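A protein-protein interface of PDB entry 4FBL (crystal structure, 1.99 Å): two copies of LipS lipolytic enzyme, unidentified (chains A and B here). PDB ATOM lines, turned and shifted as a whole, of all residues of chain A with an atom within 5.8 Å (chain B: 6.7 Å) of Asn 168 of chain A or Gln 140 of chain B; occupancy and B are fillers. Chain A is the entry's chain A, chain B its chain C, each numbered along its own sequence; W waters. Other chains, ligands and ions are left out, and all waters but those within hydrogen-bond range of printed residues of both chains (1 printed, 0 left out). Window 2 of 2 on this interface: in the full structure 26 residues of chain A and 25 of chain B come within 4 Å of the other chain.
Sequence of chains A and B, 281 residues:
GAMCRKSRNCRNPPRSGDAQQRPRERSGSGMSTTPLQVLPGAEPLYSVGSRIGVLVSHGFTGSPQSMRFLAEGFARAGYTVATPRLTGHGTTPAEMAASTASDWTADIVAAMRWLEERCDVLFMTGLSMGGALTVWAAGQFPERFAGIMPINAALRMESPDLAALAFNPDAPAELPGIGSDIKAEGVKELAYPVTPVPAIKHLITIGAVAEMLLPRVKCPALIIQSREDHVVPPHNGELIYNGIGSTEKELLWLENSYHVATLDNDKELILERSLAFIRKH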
ATOM      1  N   ALA A 163     -25.022 -17.819   4.983  1.00  0.00           N
ATOM      2  CA  ALA A 163     -25.226 -19.025   5.869  1.00  0.00           C
ATOM      3  C   ALA A 163     -23.880 -19.805   5.998  1.00  0.00           C
ATOM      4  O   ALA A 163     -23.548 -20.294   7.093  1.00  0.00           O
ATOM      5  CB  ALA A 163     -26.316 -19.935   5.328  1.00  0.00           C
ATOM      6  N   ALA A 164     -23.082 -19.852   4.922  1.00  0.00           N
ATOM      7  CA  ALA A 164     -21.768 -20.548   4.982  1.00  0.00           C
ATOM      8  C   ALA A 164     -20.754 -19.873   5.828  1.00  0.00           C
ATOM      9  O   ALA A 164     -19.671 -20.430   6.016  1.00  0.00           O
ATOM     10  CB  ALA A 164     -21.157 -20.761   3.578  1.00  0.00           C
ATOM     11  N   LEU A 165     -21.053 -18.681   6.347  1.00  0.00           N
ATOM     12  CA  LEU A 165     -20.151 -18.053   7.358  1.00  0.00           C
ATOM     13  C   LEU A 165     -20.584 -18.167   8.804  1.00  0.00           C
ATOM     14  O   LEU A 165     -19.832 -17.837   9.717  1.00  0.00           O
ATOM     15  CB  LEU A 165     -19.991 -16.560   7.028  1.00  0.00           C
ATOM     16  CG  LEU A 165     -19.257 -16.263   5.701  1.00  0.00           C
ATOM     17  CD1 LEU A 165     -19.540 -14.796   5.029  1.00  0.00           C
ATOM     18  CD2 LEU A 165     -17.755 -16.541   5.868  1.00  0.00           C
ATOM     19  N   ALA A 166     -21.820 -18.553   9.040  1.00  0.00           N
ATOM     20  CA  ALA A 166     -22.386 -18.621  10.401  1.00  0.00           C
ATOM     21  C   ALA A 166     -21.547 -19.456  11.367  1.00  0.00           C
ATOM     22  O   ALA A 166     -21.208 -18.981  12.452  1.00  0.00           O
ATOM     23  CB  ALA A 166     -23.851 -19.168  10.305  1.00  0.00           C
ATOM     24  N   PHE A 167     -21.217 -20.702  10.980  1.00  0.00           N
ATOM     25  CA  PHE A 167     -20.364 -21.641  11.795  1.00  0.00           C
ATOM     26  C   PHE A 167     -19.131 -22.231  11.042  1.00  0.00           C
ATOM     27  O   PHE A 167     -18.848 -23.440  11.130  1.00  0.00           O
ATOM     28  CB  PHE A 167     -21.292 -22.835  12.215  1.00  0.00           C
ATOM     29  CG  PHE A 167     -22.444 -22.398  13.109  1.00  0.00           C
ATOM     30  CD1 PHE A 167     -22.187 -22.020  14.412  1.00  0.00           C
ATOM     31  CD2 PHE A 167     -23.737 -22.335  12.625  1.00  0.00           C
ATOM     32  CE1 PHE A 167     -23.259 -21.574  15.323  1.00  0.00           C
ATOM     33  CE2 PHE A 167     -24.791 -21.863  13.454  1.00  0.00           C
ATOM     34  CZ  PHE A 167     -24.501 -21.484  14.851  1.00  0.00           C
ATOM     35  N   ASN A 168     -18.431 -21.408  10.285  1.00  0.00           N
ATOM     36  CA  ASN A 168     -17.349 -21.831   9.448  1.00  0.00           C
ATOM     37  C   ASN A 168     -16.171 -21.851  10.349  1.00  0.00           C
ATOM     38  O   ASN A 168     -15.808 -20.811  10.920  1.00  0.00           O
ATOM     39  CB  ASN A 168     -17.177 -20.824   8.337  1.00  0.00           C
ATOM     40  CG  ASN A 168     -16.205 -21.279   7.270  1.00  0.00           C
ATOM     41  OD1 ASN A 168     -15.383 -22.104   7.526  1.00  0.00           O
ATOM     42  ND2 ASN A 168     -16.352 -20.776   6.065  1.00  0.00           N
ATOM     43  N   PRO A 169     -15.563 -23.034  10.540  1.00  0.00           N
ATOM     44  CA  PRO A 169     -14.323 -23.070  11.386  1.00  0.00           C
ATOM     45  C   PRO A 169     -13.082 -22.416  10.720  1.00  0.00           C
ATOM     46  O   PRO A 169     -12.130 -22.091  11.412  1.00  0.00           O
ATOM     47  CB  PRO A 169     -14.066 -24.571  11.602  1.00  0.00           C
ATOM     48  CG  PRO A 169     -14.689 -25.261  10.366  1.00  0.00           C
ATOM     49  CD  PRO A 169     -15.851 -24.319   9.866  1.00  0.00           C
ATOM     50  N   ASP A 170     -13.118 -22.214   9.399  1.00  0.00           N
ATOM     51  CA  ASP A 170     -12.020 -21.606   8.612  1.00  0.00           C
ATOM     52  C   ASP A 170     -12.380 -20.276   7.967  1.00  0.00           C
ATOM     53  O   ASP A 170     -12.130 -20.111   6.740  1.00  0.00           O
ATOM     54  CB  ASP A 170     -11.701 -22.532   7.411  1.00  0.00           C
ATOM     55  CG  ASP A 170     -11.297 -23.918   7.863  1.00  0.00           C
ATOM     56  OD1 ASP A 170     -10.438 -23.927   8.806  1.00  0.00           O
ATOM     57  OD2 ASP A 170     -11.900 -24.940   7.376  1.00  0.00           O
ATOM     58  N   ALA A 171     -13.002 -19.352   8.698  1.00  0.00           N
ATOM     59  CA  ALA A 171     -13.517 -18.150   8.012  1.00  0.00           C
ATOM     60  C   ALA A 171     -12.672 -16.985   8.478  1.00  0.00           C
ATOM     61  O   ALA A 171     -12.227 -16.970   9.624  1.00  0.00           O
ATOM     62  CB  ALA A 171     -15.029 -17.914   8.377  1.00  0.00           C
ATOM     63  N   VAL B 109     -17.835 -31.099  13.506  1.00  0.00           N
ATOM     64  CA  VAL B 109     -16.528 -30.866  12.945  1.00  0.00           C
ATOM     65  C   VAL B 109     -15.479 -31.825  13.543  1.00  0.00           C
ATOM     66  O   VAL B 109     -14.767 -32.434  12.804  1.00  0.00           O
ATOM     67  CB  VAL B 109     -16.095 -29.383  13.121  1.00  0.00           C
ATOM     68  CG1 VAL B 109     -14.683 -29.234  12.612  1.00  0.00           C
ATOM     69  CG2 VAL B 109     -16.984 -28.522  12.192  1.00  0.00           C
ATOM     70  N   VAL B 135     -27.593 -31.792   7.022  1.00  0.00           N
ATOM     71  CA  VAL B 135     -27.782 -30.794   5.960  1.00  0.00           C
ATOM     72  C   VAL B 135     -26.778 -29.667   6.137  1.00  0.00           C
ATOM     73  O   VAL B 135     -26.185 -29.250   5.179  1.00  0.00           O
ATOM     74  CB  VAL B 135     -29.187 -30.246   5.900  1.00  0.00           C
ATOM     75  CG1 VAL B 135     -29.265 -29.072   4.840  1.00  0.00           C
ATOM     76  CG2 VAL B 135     -30.145 -31.354   5.490  1.00  0.00           C
ATOM     77  N   TRP B 136     -26.550 -29.200   7.351  1.00  0.00           N
ATOM     78  CA  TRP B 136     -25.596 -28.122   7.556  1.00  0.00           C
ATOM     79  C   TRP B 136     -24.217 -28.570   7.113  1.00  0.00           C
ATOM     80  O   TRP B 136     -23.482 -27.760   6.479  1.00  0.00           O
ATOM     81  CB  TRP B 136     -25.534 -27.677   9.049  1.00  0.00           C
ATOM     82  CG  TRP B 136     -24.383 -26.809   9.322  1.00  0.00           C
ATOM     83  CD1 TRP B 136     -24.291 -25.413   9.136  1.00  0.00           C
ATOM     84  CD2 TRP B 136     -23.122 -27.218   9.866  1.00  0.00           C
ATOM     85  NE1 TRP B 136     -23.027 -24.972   9.475  1.00  0.00           N
ATOM     86  CE2 TRP B 136     -22.290 -26.043   9.945  1.00  0.00           C
ATOM     87  CE3 TRP B 136     -22.617 -28.451  10.302  1.00  0.00           C
ATOM     88  CZ2 TRP B 136     -20.944 -26.080  10.400  1.00  0.00           C
ATOM     89  CZ3 TRP B 136     -21.280 -28.493  10.759  1.00  0.00           C
ATOM     90  CH2 TRP B 136     -20.463 -27.295  10.820  1.00  0.00           C
ATOM     91  N   ALA B 137     -23.799 -29.799   7.474  1.00  0.00           N
ATOM     92  CA  ALA B 137     -22.374 -30.128   7.148  1.00  0.00           C
ATOM     93  C   ALA B 137     -22.175 -30.362   5.618  1.00  0.00           C
ATOM     94  O   ALA B 137     -21.136 -29.975   5.089  1.00  0.00           O
ATOM     95  CB  ALA B 137     -21.893 -31.380   7.937  1.00  0.00           C
ATOM     96  N   ALA B 138     -23.160 -30.925   4.919  1.00  0.00           N
ATOM     97  CA  ALA B 138     -23.084 -31.127   3.490  1.00  0.00           C
ATOM     98  C   ALA B 138     -23.126 -29.790   2.683  1.00  0.00           C
ATOM     99  O   ALA B 138     -22.597 -29.741   1.551  1.00  0.00           O
ATOM    100  CB  ALA B 138     -24.207 -32.080   2.991  1.00  0.00           C
ATOM    101  N   GLY B 139     -23.750 -28.739   3.264  1.00  0.00           N
ATOM    102  CA  GLY B 139     -23.792 -27.374   2.670  1.00  0.00           C
ATOM    103  C   GLY B 139     -22.543 -26.555   3.011  1.00  0.00           C
ATOM    104  O   GLY B 139     -22.028 -25.737   2.196  1.00  0.00           O
ATOM    105  N   GLN B 140     -22.019 -26.814   4.186  1.00  0.00           N
ATOM    106  CA  GLN B 140     -20.880 -26.076   4.744  1.00  0.00           C
ATOM    107  C   GLN B 140     -19.583 -26.562   4.118  1.00  0.00           C
ATOM    108  O   GLN B 140     -18.651 -25.715   3.889  1.00  0.00           O
ATOM    109  CB  GLN B 140     -20.772 -26.262   6.246  1.00  0.00           C
ATOM    110  CG  GLN B 140     -19.584 -25.613   6.884  1.00  0.00           C
ATOM    111  CD  GLN B 140     -19.660 -24.024   6.806  1.00  0.00           C
ATOM    112  OE1 GLN B 140     -20.341 -23.405   7.576  1.00  0.00           O
ATOM    113  NE2 GLN B 140     -18.967 -23.423   5.858  1.00  0.00           N
ATOM    114  N   PHE B 141     -19.526 -27.878   3.819  1.00  0.00           N
ATOM    115  CA  PHE B 141     -18.300 -28.539   3.233  1.00  0.00           C
ATOM    116  C   PHE B 141     -18.788 -29.325   2.027  1.00  0.00           C
ATOM    117  O   PHE B 141     -18.971 -30.544   2.097  1.00  0.00           O
ATOM    118  CB  PHE B 141     -17.734 -29.507   4.227  1.00  0.00           C
ATOM    119  CG  PHE B 141     -17.398 -28.857   5.565  1.00  0.00           C
ATOM    120  CD1 PHE B 141     -16.208 -28.081   5.727  1.00  0.00           C
ATOM    121  CD2 PHE B 141     -18.285 -28.983   6.657  1.00  0.00           C
ATOM    122  CE1 PHE B 141     -15.923 -27.460   7.002  1.00  0.00           C
ATOM    123  CE2 PHE B 141     -18.003 -28.422   7.927  1.00  0.00           C
ATOM    124  CZ  PHE B 141     -16.833 -27.653   8.113  1.00  0.00           C
ATOM    125  N   PRO B 142     -19.089 -28.626   0.947  1.00  0.00           N
ATOM    126  CA  PRO B 142     -19.846 -29.228  -0.122  1.00  0.00           C
ATOM    127  C   PRO B 142     -19.163 -30.357  -0.894  1.00  0.00           C
ATOM    128  O   PRO B 142     -19.831 -31.040  -1.593  1.00  0.00           O
ATOM    129  CB  PRO B 142     -20.079 -28.040  -1.098  1.00  0.00           C
ATOM    130  CG  PRO B 142     -19.690 -26.830  -0.393  1.00  0.00           C
ATOM    131  CD  PRO B 142     -18.677 -27.250   0.615  1.00  0.00           C
ATOM    132  N   GLU B 143     -17.859 -30.540  -0.768  1.00  0.00           N
ATOM    133  CA  GLU B 143     -17.192 -31.597  -1.518  1.00  0.00           C
ATOM    134  C   GLU B 143     -16.842 -32.713  -0.573  1.00  0.00           C
ATOM    135  O   GLU B 143     -16.167 -33.664  -0.985  1.00  0.00           O
ATOM    136  CB  GLU B 143     -15.809 -31.121  -2.045  1.00  0.00           C
ATOM    137  CG  GLU B 143     -15.810 -29.766  -2.631  1.00  0.00           C
ATOM    138  CD  GLU B 143     -16.013 -29.806  -4.104  1.00  0.00           C
ATOM    139  OE1 GLU B 143     -16.976 -30.419  -4.592  1.00  0.00           O
ATOM    140  OE2 GLU B 143     -15.183 -29.212  -4.795  1.00  0.00           O
ATOM    141  N   VAL B 209     -29.897 -22.019   9.626  1.00  0.00           N
ATOM    142  CA  VAL B 209     -28.639 -21.995   8.891  1.00  0.00           C
ATOM    143  C   VAL B 209     -28.682 -23.124   7.857  1.00  0.00           C
ATOM    144  O   VAL B 209     -28.383 -22.910   6.672  1.00  0.00           O
ATOM    145  CB  VAL B 209     -27.407 -22.053   9.802  1.00  0.00           C
ATOM    146  CG1 VAL B 209     -26.093 -22.318   8.942  1.00  0.00           C
ATOM    147  CG2 VAL B 209     -27.304 -20.713  10.620  1.00  0.00           C
ATOM    148  N   LEU B 213     -28.417 -22.911   3.681  1.00  0.00           N
ATOM    149  CA  LEU B 213     -27.419 -23.671   2.909  1.00  0.00           C
ATOM    150  C   LEU B 213     -27.911 -24.676   1.834  1.00  0.00           C
ATOM    151  O   LEU B 213     -27.113 -25.131   0.998  1.00  0.00           O
ATOM    152  CB  LEU B 213     -26.566 -24.452   3.874  1.00  0.00           C
ATOM    153  CG  LEU B 213     -25.652 -23.630   4.730  1.00  0.00           C
ATOM    154  CD1 LEU B 213     -24.915 -24.500   5.835  1.00  0.00           C
ATOM    155  CD2 LEU B 213     -24.564 -22.990   3.857  1.00  0.00           C
ATOM    156  N   ARG B 216     -26.481 -25.101  -1.699  1.00  0.00           N
ATOM    157  CA  ARG B 216     -25.105 -25.583  -1.700  1.00  0.00           C
ATOM    158  C   ARG B 216     -24.882 -27.066  -1.496  1.00  0.00           C
ATOM    159  O   ARG B 216     -23.761 -27.568  -1.744  1.00  0.00           O
ATOM    160  CB  ARG B 216     -24.361 -24.913  -0.603  1.00  0.00           C
ATOM    161  CG  ARG B 216     -23.798 -23.549  -0.903  1.00  0.00           C
ATOM    162  CD  ARG B 216     -23.278 -23.155   0.435  1.00  0.00           C
ATOM    163  NE  ARG B 216     -22.146 -22.288   0.357  1.00  0.00           N
ATOM    164  CZ  ARG B 216     -20.901 -22.523   0.759  1.00  0.00           C
ATOM    165  NH1 ARG B 216     -20.476 -23.654   1.313  1.00  0.00           N
ATOM    166  NH2 ARG B 216     -20.067 -21.510   0.589  1.00  0.00           N
ATOM    167  N   VAL B 217     -25.907 -27.783  -1.062  1.00  0.00           N
ATOM    168  CA  VAL B 217     -25.766 -29.252  -0.887  1.00  0.00           C
ATOM    169  C   VAL B 217     -25.815 -29.900  -2.264  1.00  0.00           C
ATOM    170  O   VAL B 217     -26.790 -29.693  -2.956  1.00  0.00           O
ATOM    171  CB  VAL B 217     -26.917 -29.874  -0.068  1.00  0.00           C
ATOM    172  CG1 VAL B 217     -26.743 -31.380  -0.011  1.00  0.00           C
ATOM    173  CG2 VAL B 217     -26.956 -29.270   1.350  1.00  0.00           C
HETATM  174  O   HOH W   1     -22.134 -22.131   8.779  1.00  0.00           O
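The backbone carbonyl oxygen (O) of Ala 164 of chain A sits at hydrogen-bond distance from the side-chain amide nitrogen (NE2) of Gln 140 of chain B (3.1 Å).
Water W1 lies within hydrogen-bond range of the side-chain amide oxygen (OE1) of Gln 140 of chain B, the backbone NH (N) of Phe 167 of chain A, the backbone carbonyl oxygen (O) of Ala 163 of chain A and the indole nitrogen (NE1) of Trp 136 of chain B.
Ala 163 of chain A touches Val 209 of chain B (O to CG1, 3.7 Å).
Leu 213 of chain B touches Ala 163 of chain A (CG to CB, 3.8 Å).
Leu 213 of chain B touches Ala 164 of chain A.
Ala 164 of chain A touches Arg 216 of chain B.
Val 209 of chain B touches Ala 166 of chain A.
Trp 136 of chain B touches Phe 167 of chain A.
Phe 167 of chain A touches Gln 140 of chain B (C to OE1, 3.9 Å).
Phe 167 of chain A touches Val 209 of chain B.
Asn 168 of chain A touches Gln 140 of chain B (ND2 to NE2, 3.7 Å).
Phe 141 of chain B touches Pro 169 of chain A (CZ to CD, 3.9 Å).
O of Ala 164 of chain A is in hydrogen-bond range of ND2 of Asn 168 of chain A, at 3.3 Å.
The side-chain amide oxygen (OD1) of Asn 168 of chain A sits at hydrogen-bond distance from the backbone NH (N) of Asp 170 of chain A, at 2.9 Å.
The guanidinium group of Arg 216 of chain B lies within hydrogen-bond range of the backbone carbonyl oxygen of Gly 139 of chain B (2.7 Å).
Gln 140 of chain B touches just these residues of chain A: Ala 164 (3.1 Å), Phe 167 (3.9 Å) and Asn 168 (3.7 Å).
Printed residues of chain A within 4 Å of Trp 136 of chain B: Phe 167.
Printed residues of chain B within 4 Å of Ala 166 of chain A: Val 209.
Printed residues of chain B within 4 Å of Pro 169 of chain A: Phe 141 (3.9 Å).
Gly 139 of chain B touches none of the printed residues of chain A.
Val 217 of chain B touches none of the printed residues of chain A.
The nearest residue of chain A that does not touch Gln 140 of chain B is Ala 163 of chain A (4.5 Å).
The nearest printed residue of chain B that does not touch Pro 169 of chain A is Val 109 of chain B (4.4 Å).
No position is printed for both chains.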
